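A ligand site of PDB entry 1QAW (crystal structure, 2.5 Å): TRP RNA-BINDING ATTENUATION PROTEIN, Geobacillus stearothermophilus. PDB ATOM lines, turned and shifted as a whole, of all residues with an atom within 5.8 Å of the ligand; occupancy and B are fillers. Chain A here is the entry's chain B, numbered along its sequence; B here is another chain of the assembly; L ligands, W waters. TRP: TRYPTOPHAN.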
ATOM      1  N   LEU A  22     -30.514  13.354  -6.077  1.00  0.00           N
ATOM      2  CA  LEU A  22     -30.594  13.620  -4.650  1.00  0.00           C
ATOM      3  C   LEU A  22     -29.447  14.546  -4.283  1.00  0.00           C
ATOM      4  O   LEU A  22     -28.410  14.402  -4.894  1.00  0.00           O
ATOM      5  CB  LEU A  22     -30.538  12.374  -3.747  1.00  0.00           C
ATOM      6  CG  LEU A  22     -31.855  11.591  -3.722  1.00  0.00           C
ATOM      7  CD1 LEU A  22     -32.250  11.166  -5.141  1.00  0.00           C
ATOM      8  CD2 LEU A  22     -31.777  10.340  -2.849  1.00  0.00           C
ATOM      9  N   THR A  23     -29.729  15.613  -3.583  1.00  0.00           N
ATOM     10  CA  THR A  23     -28.712  16.617  -3.328  1.00  0.00           C
ATOM     11  C   THR A  23     -27.565  16.074  -2.447  1.00  0.00           C
ATOM     12  O   THR A  23     -27.694  15.383  -1.456  1.00  0.00           O
ATOM     13  CB  THR A  23     -29.357  17.807  -2.552  1.00  0.00           C
ATOM     14  OG1 THR A  23     -29.983  17.189  -1.420  1.00  0.00           O
ATOM     15  CG2 THR A  23     -30.386  18.583  -3.323  1.00  0.00           C
ATOM     16  N   ARG A  24     -26.379  16.575  -2.744  1.00  0.00           N
ATOM     17  CA  ARG A  24     -25.180  16.375  -2.009  1.00  0.00           C
ATOM     18  C   ARG A  24     -25.148  17.207  -0.741  1.00  0.00           C
ATOM     19  O   ARG A  24     -25.570  18.353  -0.937  1.00  0.00           O
ATOM     20  CB  ARG A  24     -23.969  16.826  -2.840  1.00  0.00           C
ATOM     21  CG  ARG A  24     -22.731  16.472  -2.000  1.00  0.00           C
ATOM     22  CD  ARG A  24     -21.491  16.712  -2.846  1.00  0.00           C
ATOM     23  NE  ARG A  24     -21.416  15.806  -3.972  1.00  0.00           N
ATOM     24  CZ  ARG A  24     -20.927  14.567  -4.008  1.00  0.00           C
ATOM     25  NH1 ARG A  24     -20.428  14.049  -2.872  1.00  0.00           N
ATOM     26  NH2 ARG A  24     -20.946  13.922  -5.190  1.00  0.00           N
ATOM     27  N   GLY A  25     -24.848  16.724   0.459  1.00  0.00           N
ATOM     28  CA  GLY A  25     -24.597  17.676   1.531  1.00  0.00           C
ATOM     29  C   GLY A  25     -25.277  17.112   2.764  1.00  0.00           C
ATOM     30  O   GLY A  25     -25.784  15.977   2.694  1.00  0.00           O
ATOM     31  N   ALA A  26     -25.278  17.919   3.859  1.00  0.00           N
ATOM     32  CA  ALA A  26     -25.993  17.423   5.028  1.00  0.00           C
ATOM     33  C   ALA A  26     -27.477  17.137   4.811  1.00  0.00           C
ATOM     34  O   ALA A  26     -28.092  16.523   5.696  1.00  0.00           O
ATOM     35  CB  ALA A  26     -25.854  18.357   6.234  1.00  0.00           C
ATOM     36  N   ASP A  27     -28.183  17.742   3.871  1.00  0.00           N
ATOM     37  CA  ASP A  27     -29.626  17.464   3.733  1.00  0.00           C
ATOM     38  C   ASP A  27     -29.821  16.625   2.482  1.00  0.00           C
ATOM     39  O   ASP A  27     -29.007  16.806   1.579  1.00  0.00           O
ATOM     40  CB  ASP A  27     -30.464  18.777   3.533  1.00  0.00           C
ATOM     41  CG  ASP A  27     -30.438  19.423   4.922  1.00  0.00           C
ATOM     42  OD1 ASP A  27     -30.847  18.724   5.900  1.00  0.00           O
ATOM     43  OD2 ASP A  27     -29.909  20.544   4.926  1.00  0.00           O
ATOM     44  N   THR A  28     -30.895  15.878   2.556  1.00  0.00           N
ATOM     45  CA  THR A  28     -31.169  15.025   1.395  1.00  0.00           C
ATOM     46  C   THR A  28     -32.596  15.188   0.853  1.00  0.00           C
ATOM     47  O   THR A  28     -33.587  14.754   1.486  1.00  0.00           O
ATOM     48  CB  THR A  28     -30.936  13.531   1.748  1.00  0.00           C
ATOM     49  OG1 THR A  28     -29.701  13.364   2.404  1.00  0.00           O
ATOM     50  CG2 THR A  28     -30.877  12.776   0.402  1.00  0.00           C
ATOM     51  N   SER A  51     -25.336  13.451  -5.401  1.00  0.00           N
ATOM     52  CA  SER A  51     -24.597  12.356  -4.817  1.00  0.00           C
ATOM     53  C   SER A  51     -25.464  11.091  -4.673  1.00  0.00           C
ATOM     54  O   SER A  51     -24.911  10.131  -4.086  1.00  0.00           O
ATOM     55  CB  SER A  51     -23.947  12.757  -3.470  1.00  0.00           C
ATOM     56  OG  SER A  51     -25.025  13.109  -2.567  1.00  0.00           O
ATOM     57  N   ALA A  52     -26.735  11.099  -5.110  1.00  0.00           N
ATOM     58  CA  ALA A  52     -27.433   9.806  -5.148  1.00  0.00           C
ATOM     59  C   ALA A  52     -28.487   9.877  -6.255  1.00  0.00           C
ATOM     60  O   ALA A  52     -28.914  10.962  -6.615  1.00  0.00           O
ATOM     61  CB  ALA A  52     -28.059   9.354  -3.838  1.00  0.00           C
ATOM     62  N   VAL B  19     -32.591   2.382   2.688  1.00  0.00           N
ATOM     63  CA  VAL B  19     -31.151   2.651   2.515  1.00  0.00           C
ATOM     64  C   VAL B  19     -30.751   3.812   3.401  1.00  0.00           C
ATOM     65  O   VAL B  19     -31.127   4.952   3.062  1.00  0.00           O
ATOM     66  CB  VAL B  19     -30.917   2.942   1.013  1.00  0.00           C
ATOM     67  CG1 VAL B  19     -29.428   3.057   0.752  1.00  0.00           C
ATOM     68  CG2 VAL B  19     -31.422   1.740   0.192  1.00  0.00           C
ATOM     69  N   ILE B  20     -30.208   3.620   4.588  1.00  0.00           N
ATOM     70  CA  ILE B  20     -29.825   4.585   5.609  1.00  0.00           C
ATOM     71  C   ILE B  20     -28.348   5.015   5.551  1.00  0.00           C
ATOM     72  O   ILE B  20     -27.394   4.238   5.660  1.00  0.00           O
ATOM     73  CB  ILE B  20     -29.983   3.906   6.990  1.00  0.00           C
ATOM     74  CG1 ILE B  20     -31.267   3.060   7.009  1.00  0.00           C
ATOM     75  CG2 ILE B  20     -29.886   4.688   8.328  1.00  0.00           C
ATOM     76  CD1 ILE B  20     -31.367   2.222   8.275  1.00  0.00           C
ATOM     77  N   GLY B  21     -28.020   6.288   5.442  1.00  0.00           N
ATOM     78  CA  GLY B  21     -26.729   6.898   5.460  1.00  0.00           C
ATOM     79  C   GLY B  21     -26.372   7.202   6.922  1.00  0.00           C
ATOM     80  O   GLY B  21     -27.203   7.786   7.629  1.00  0.00           O
ATOM     81  N   LEU B  22     -25.114   6.867   7.288  1.00  0.00           N
ATOM     82  CA  LEU B  22     -24.577   7.156   8.614  1.00  0.00           C
ATOM     83  C   LEU B  22     -23.564   8.281   8.479  1.00  0.00           C
ATOM     84  O   LEU B  22     -22.793   8.400   7.498  1.00  0.00           O
ATOM     85  CB  LEU B  22     -23.907   5.897   9.188  1.00  0.00           C
ATOM     86  CG  LEU B  22     -24.768   4.740   9.630  1.00  0.00           C
ATOM     87  CD1 LEU B  22     -25.400   3.988   8.476  1.00  0.00           C
ATOM     88  CD2 LEU B  22     -24.075   3.618  10.463  1.00  0.00           C
ATOM     89  N   HIS B  31     -28.436   9.924   9.424  1.00  0.00           N
ATOM     90  CA  HIS B  31     -28.779  11.292   9.085  1.00  0.00           C
ATOM     91  C   HIS B  31     -29.888  11.250   8.014  1.00  0.00           C
ATOM     92  O   HIS B  31     -30.532  12.267   7.817  1.00  0.00           O
ATOM     93  CB  HIS B  31     -27.680  12.207   8.574  1.00  0.00           C
ATOM     94  CG  HIS B  31     -26.987  11.705   7.335  1.00  0.00           C
ATOM     95  ND1 HIS B  31     -27.386  12.036   6.067  1.00  0.00           N
ATOM     96  CD2 HIS B  31     -25.942  10.845   7.166  1.00  0.00           C
ATOM     97  CE1 HIS B  31     -26.606  11.457   5.153  1.00  0.00           C
ATOM     98  NE2 HIS B  31     -25.710  10.730   5.818  1.00  0.00           N
ATOM     99  N   HIS B  32     -30.181  10.130   7.366  1.00  0.00           N
ATOM    100  CA  HIS B  32     -31.136  10.086   6.291  1.00  0.00           C
ATOM    101  C   HIS B  32     -31.534   8.621   6.023  1.00  0.00           C
ATOM    102  O   HIS B  32     -30.669   7.744   6.125  1.00  0.00           O
ATOM    103  CB  HIS B  32     -30.593  10.639   4.979  1.00  0.00           C
ATOM    104  CG  HIS B  32     -31.608  10.584   3.895  1.00  0.00           C
ATOM    105  ND1 HIS B  32     -32.926  11.024   4.064  1.00  0.00           N
ATOM    106  CD2 HIS B  32     -31.545  10.198   2.601  1.00  0.00           C
ATOM    107  CE1 HIS B  32     -33.584  10.867   2.943  1.00  0.00           C
ATOM    108  NE2 HIS B  32     -32.790  10.367   2.025  1.00  0.00           N
ATOM    109  N   SER B  33     -32.821   8.466   5.759  1.00  0.00           N
ATOM    110  CA  SER B  33     -33.339   7.148   5.406  1.00  0.00           C
ATOM    111  C   SER B  33     -34.168   7.173   4.131  1.00  0.00           C
ATOM    112  O   SER B  33     -35.055   8.016   4.075  1.00  0.00           O
ATOM    113  CB  SER B  33     -34.190   6.765   6.598  1.00  0.00           C
ATOM    114  OG  SER B  33     -34.514   5.401   6.515  1.00  0.00           O
ATOM    115  N   GLU B  34     -33.753   6.646   2.997  1.00  0.00           N
ATOM    116  CA  GLU B  34     -34.485   6.619   1.771  1.00  0.00           C
ATOM    117  C   GLU B  34     -35.250   5.289   1.629  1.00  0.00           C
ATOM    118  O   GLU B  34     -34.700   4.193   1.712  1.00  0.00           O
ATOM    119  CB  GLU B  34     -33.672   6.796   0.504  1.00  0.00           C
ATOM    120  CG  GLU B  34     -34.566   7.061  -0.691  1.00  0.00           C
ATOM    121  CD  GLU B  34     -34.686   8.569  -0.964  1.00  0.00           C
ATOM    122  OE1 GLU B  34     -34.356   9.313   0.002  1.00  0.00           O
ATOM    123  OE2 GLU B  34     -35.030   8.879  -2.135  1.00  0.00           O
ATOM    124  N   LEU B  42     -31.781   2.533  -6.324  1.00  0.00           N
ATOM    125  CA  LEU B  42     -31.071   3.700  -5.778  1.00  0.00           C
ATOM    126  C   LEU B  42     -29.580   3.525  -6.046  1.00  0.00           C
ATOM    127  O   LEU B  42     -29.013   2.417  -6.015  1.00  0.00           O
ATOM    128  CB  LEU B  42     -31.319   3.880  -4.266  1.00  0.00           C
ATOM    129  CG  LEU B  42     -30.496   5.052  -3.647  1.00  0.00           C
ATOM    130  CD1 LEU B  42     -30.955   6.382  -4.228  1.00  0.00           C
ATOM    131  CD2 LEU B  42     -30.731   5.162  -2.131  1.00  0.00           C
ATOM    132  N   ALA B  44     -26.144   5.114  -4.878  1.00  0.00           N
ATOM    133  CA  ALA B  44     -25.700   6.125  -3.923  1.00  0.00           C
ATOM    134  C   ALA B  44     -24.201   6.054  -3.649  1.00  0.00           C
ATOM    135  O   ALA B  44     -23.605   4.976  -3.403  1.00  0.00           O
ATOM    136  CB  ALA B  44     -26.506   6.002  -2.612  1.00  0.00           C
ATOM    137  N   GLN B  45     -23.632   7.257  -3.513  1.00  0.00           N
ATOM    138  CA  GLN B  45     -22.176   7.383  -3.317  1.00  0.00           C
ATOM    139  C   GLN B  45     -21.760   7.650  -1.865  1.00  0.00           C
ATOM    140  O   GLN B  45     -22.646   7.906  -1.047  1.00  0.00           O
ATOM    141  CB  GLN B  45     -21.716   8.545  -4.140  1.00  0.00           C
ATOM    142  CG  GLN B  45     -21.436   8.406  -5.627  1.00  0.00           C
ATOM    143  CD  GLN B  45     -20.674   9.710  -5.981  1.00  0.00           C
ATOM    144  OE1 GLN B  45     -21.105  10.819  -5.664  1.00  0.00           O
ATOM    145  NE2 GLN B  45     -19.510   9.499  -6.574  1.00  0.00           N
ATOM    146  N   PHE B  46     -20.496   7.252  -1.583  1.00  0.00           N
ATOM    147  CA  PHE B  46     -19.959   7.650  -0.279  1.00  0.00           C
ATOM    148  C   PHE B  46     -19.512   9.116  -0.405  1.00  0.00           C
ATOM    149  O   PHE B  46     -19.052   9.527  -1.480  1.00  0.00           O
ATOM    150  CB  PHE B  46     -18.772   6.857   0.266  1.00  0.00           C
ATOM    151  CG  PHE B  46     -19.116   5.429   0.553  1.00  0.00           C
ATOM    152  CD1 PHE B  46     -19.769   5.067   1.691  1.00  0.00           C
ATOM    153  CD2 PHE B  46     -18.755   4.438  -0.364  1.00  0.00           C
ATOM    154  CE1 PHE B  46     -20.113   3.750   1.986  1.00  0.00           C
ATOM    155  CE2 PHE B  46     -19.068   3.122  -0.060  1.00  0.00           C
ATOM    156  CZ  PHE B  46     -19.748   2.765   1.091  1.00  0.00           C
ATOM    157  N   THR B  47     -19.857   9.946   0.552  1.00  0.00           N
ATOM    158  CA  THR B  47     -19.579  11.385   0.323  1.00  0.00           C
ATOM    159  C   THR B  47     -18.946  12.015   1.564  1.00  0.00           C
ATOM    160  O   THR B  47     -18.829  11.354   2.643  1.00  0.00           O
ATOM    161  CB  THR B  47     -20.978  12.057   0.152  1.00  0.00           C
ATOM    162  OG1 THR B  47     -21.608  11.904   1.458  1.00  0.00           O
ATOM    163  CG2 THR B  47     -21.980  11.353  -0.768  1.00  0.00           C
ATOM    164  N   GLU B  48     -18.966  13.329   1.599  1.00  0.00           N
ATOM    165  CA  GLU B  48     -18.521  14.068   2.763  1.00  0.00           C
ATOM    166  C   GLU B  48     -19.460  13.916   3.969  1.00  0.00           C
ATOM    167  O   GLU B  48     -19.088  14.096   5.151  1.00  0.00           O
ATOM    168  CB  GLU B  48     -18.415  15.532   2.353  1.00  0.00           C
ATOM    169  CG  GLU B  48     -18.332  16.476   3.538  1.00  0.00           C
ATOM    170  CD  GLU B  48     -18.051  17.901   3.086  1.00  0.00           C
ATOM    171  OE1 GLU B  48     -17.438  18.113   1.997  1.00  0.00           O
ATOM    172  OE2 GLU B  48     -18.467  18.793   3.863  1.00  0.00           O
ATOM    173  N   HIS B  49     -20.742  13.656   3.690  1.00  0.00           N
ATOM    174  CA  HIS B  49     -21.612  13.476   4.841  1.00  0.00           C
ATOM    175  C   HIS B  49     -21.821  12.005   5.068  1.00  0.00           C
ATOM    176  O   HIS B  49     -22.335  11.674   6.131  1.00  0.00           O
ATOM    177  CB  HIS B  49     -22.909  14.281   4.682  1.00  0.00           C
ATOM    178  CG  HIS B  49     -22.604  15.747   4.753  1.00  0.00           C
ATOM    179  ND1 HIS B  49     -22.080  16.343   3.615  1.00  0.00           N
ATOM    180  CD2 HIS B  49     -22.667  16.671   5.728  1.00  0.00           C
ATOM    181  CE1 HIS B  49     -21.844  17.635   3.912  1.00  0.00           C
ATOM    182  NE2 HIS B  49     -22.202  17.853   5.168  1.00  0.00           N
ATOM    183  N   THR B  50     -21.465  11.094   4.162  1.00  0.00           N
ATOM    184  CA  THR B  50     -21.825   9.680   4.419  1.00  0.00           C
ATOM    185  C   THR B  50     -20.644   8.708   4.226  1.00  0.00           C
ATOM    186  O   THR B  50     -20.035   8.679   3.164  1.00  0.00           O
ATOM    187  CB  THR B  50     -22.936   9.253   3.443  1.00  0.00           C
ATOM    188  OG1 THR B  50     -24.089  10.049   3.659  1.00  0.00           O
ATOM    189  CG2 THR B  50     -23.272   7.772   3.684  1.00  0.00           C
ATOM    190  N   ILE B  53     -23.133   2.958   4.880  1.00  0.00           N
ATOM    191  CA  ILE B  53     -24.477   2.795   4.409  1.00  0.00           C
ATOM    192  C   ILE B  53     -25.089   1.475   4.891  1.00  0.00           C
ATOM    193  O   ILE B  53     -24.455   0.456   4.690  1.00  0.00           O
ATOM    194  CB  ILE B  53     -24.511   2.921   2.863  1.00  0.00           C
ATOM    195  CG1 ILE B  53     -24.048   4.279   2.356  1.00  0.00           C
ATOM    196  CG2 ILE B  53     -25.886   2.688   2.276  1.00  0.00           C
ATOM    197  CD1 ILE B  53     -23.707   4.310   0.905  1.00  0.00           C
HETATM  198  N   TRP L   1     -27.326  14.085   1.166  1.00  0.00           N
HETATM  199  CA  TRP L   1     -26.558  12.882   1.062  1.00  0.00           C
HETATM  200  C   TRP L   1     -25.044  12.943   0.882  1.00  0.00           C
HETATM  201  O   TRP L   1     -24.574  13.782   0.107  1.00  0.00           O
HETATM  202  CB  TRP L   1     -27.087  11.908   0.042  1.00  0.00           C
HETATM  203  CG  TRP L   1     -26.555  10.512   0.069  1.00  0.00           C
HETATM  204  CD1 TRP L   1     -25.557   9.993  -0.711  1.00  0.00           C
HETATM  205  CD2 TRP L   1     -27.070   9.452   0.853  1.00  0.00           C
HETATM  206  NE1 TRP L   1     -25.443   8.659  -0.461  1.00  0.00           N
HETATM  207  CE2 TRP L   1     -26.334   8.299   0.516  1.00  0.00           C
HETATM  208  CE3 TRP L   1     -28.077   9.359   1.835  1.00  0.00           C
HETATM  209  CZ2 TRP L   1     -26.540   7.059   1.127  1.00  0.00           C
HETATM  210  CZ3 TRP L   1     -28.281   8.133   2.428  1.00  0.00           C
HETATM  211  CH2 TRP L   1     -27.534   6.996   2.054  1.00  0.00           C
HETATM  212  OXT TRP L   1     -24.364  12.183   1.634  1.00  0.00           O
HETATM  213  O   HOH W   1     -21.943  15.148   1.219  1.00  0.00           O
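The backbone carbonyl oxygen (O) of Gly 21 of chain B lies within hydrogen-bond range of the backbone NH (N) of His 31 of chain B, at 3.1 Å. A ring nitrogen (NE2) of His 31 of chain B lies within hydrogen-bond range of the side-chain hydroxyl (OG1) of Thr 50 of chain B (2.8 Å). The side-chain hydroxyl (OG1) of Thr 47 of chain B sits at hydrogen-bond distance from the backbone NH (N) of Thr 50 of chain B, at 2.8 Å. The side-chain hydroxyl of Thr 23 is in hydrogen-bond range of the backbone carbonyl oxygen of Asp 27 (3.2 Å). N of Ala 26 is in hydrogen-bond range of NE2 of His 49 of chain B (3.3 Å). The side-chain amide oxygen (OE1) of Gln 45 of chain B sits at hydrogen-bond distance from the guanidinium group (NH2) of Arg 24, at 3.1 Å. The backbone carbonyl oxygen (O) of His 32 of chain B sits at hydrogen-bond distance from the backbone NH (N) of Gly 21 of chain B (3.1 Å). OG1 of Thr 47 of chain B lies within hydrogen-bond range of N of His 49 of chain B, 3.0 Å away.
Arg 24 touches the ligand (CA to O, 3.4 Å). N of Gly 21 of chain B touches CH2 of the ligand (3.5 Å). His 32 of chain B touches the ligand (CD2 to CE3, 3.6 Å). CB of Ala 44 of chain B touches NE1 of the ligand (3.6 Å). CB of His 49 of chain B touches OXT of the ligand, 3.98 Å away. CG1 of Ile 53 of chain B touches CZ2 of the ligand (3.9 Å). Of the 26 residues printed, 14 come within 4 Å of the ligand.
The side-chain hydroxyl of Thr 50 of chain B is in hydrogen-bond range of an oxygen (OXT) of the ligand (3.0 Å). The backbone carbonyl oxygen of Gln 45 of chain B sits at hydrogen-bond distance from a nitrogen (NE1) of the ligand (3.0 Å). A nitrogen (N) of the ligand is in hydrogen-bond range of the backbone carbonyl oxygen (O) of Asp 27, at 3.2 Å. A nitrogen (N) of the ligand lies within hydrogen-bond range of the backbone carbonyl oxygen of Gly 25, 2.9 Å away. O of Thr 23 sits at hydrogen-bond distance from N of the ligand, 2.9 Å away. The side-chain hydroxyl of Ser 51 is in hydrogen-bond range of an oxygen (O) of the ligand. OXT of the ligand sits at hydrogen-bond distance from OG1 of Thr 47 of chain B, 2.8 Å away. A nitrogen (N) of the ligand is in hydrogen-bond range of the side-chain hydroxyl (OG1) of Thr 28, 2.8 Å away. The backbone NH of Gly 25 lies within hydrogen-bond range of an oxygen (O) of the ligand, at 3.0 Å.
Water W1 lies within hydrogen-bond range of ND1 of His 49 of chain B, O of the ligand, OG1 of Thr 47 of chain B and N of Gly 25.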
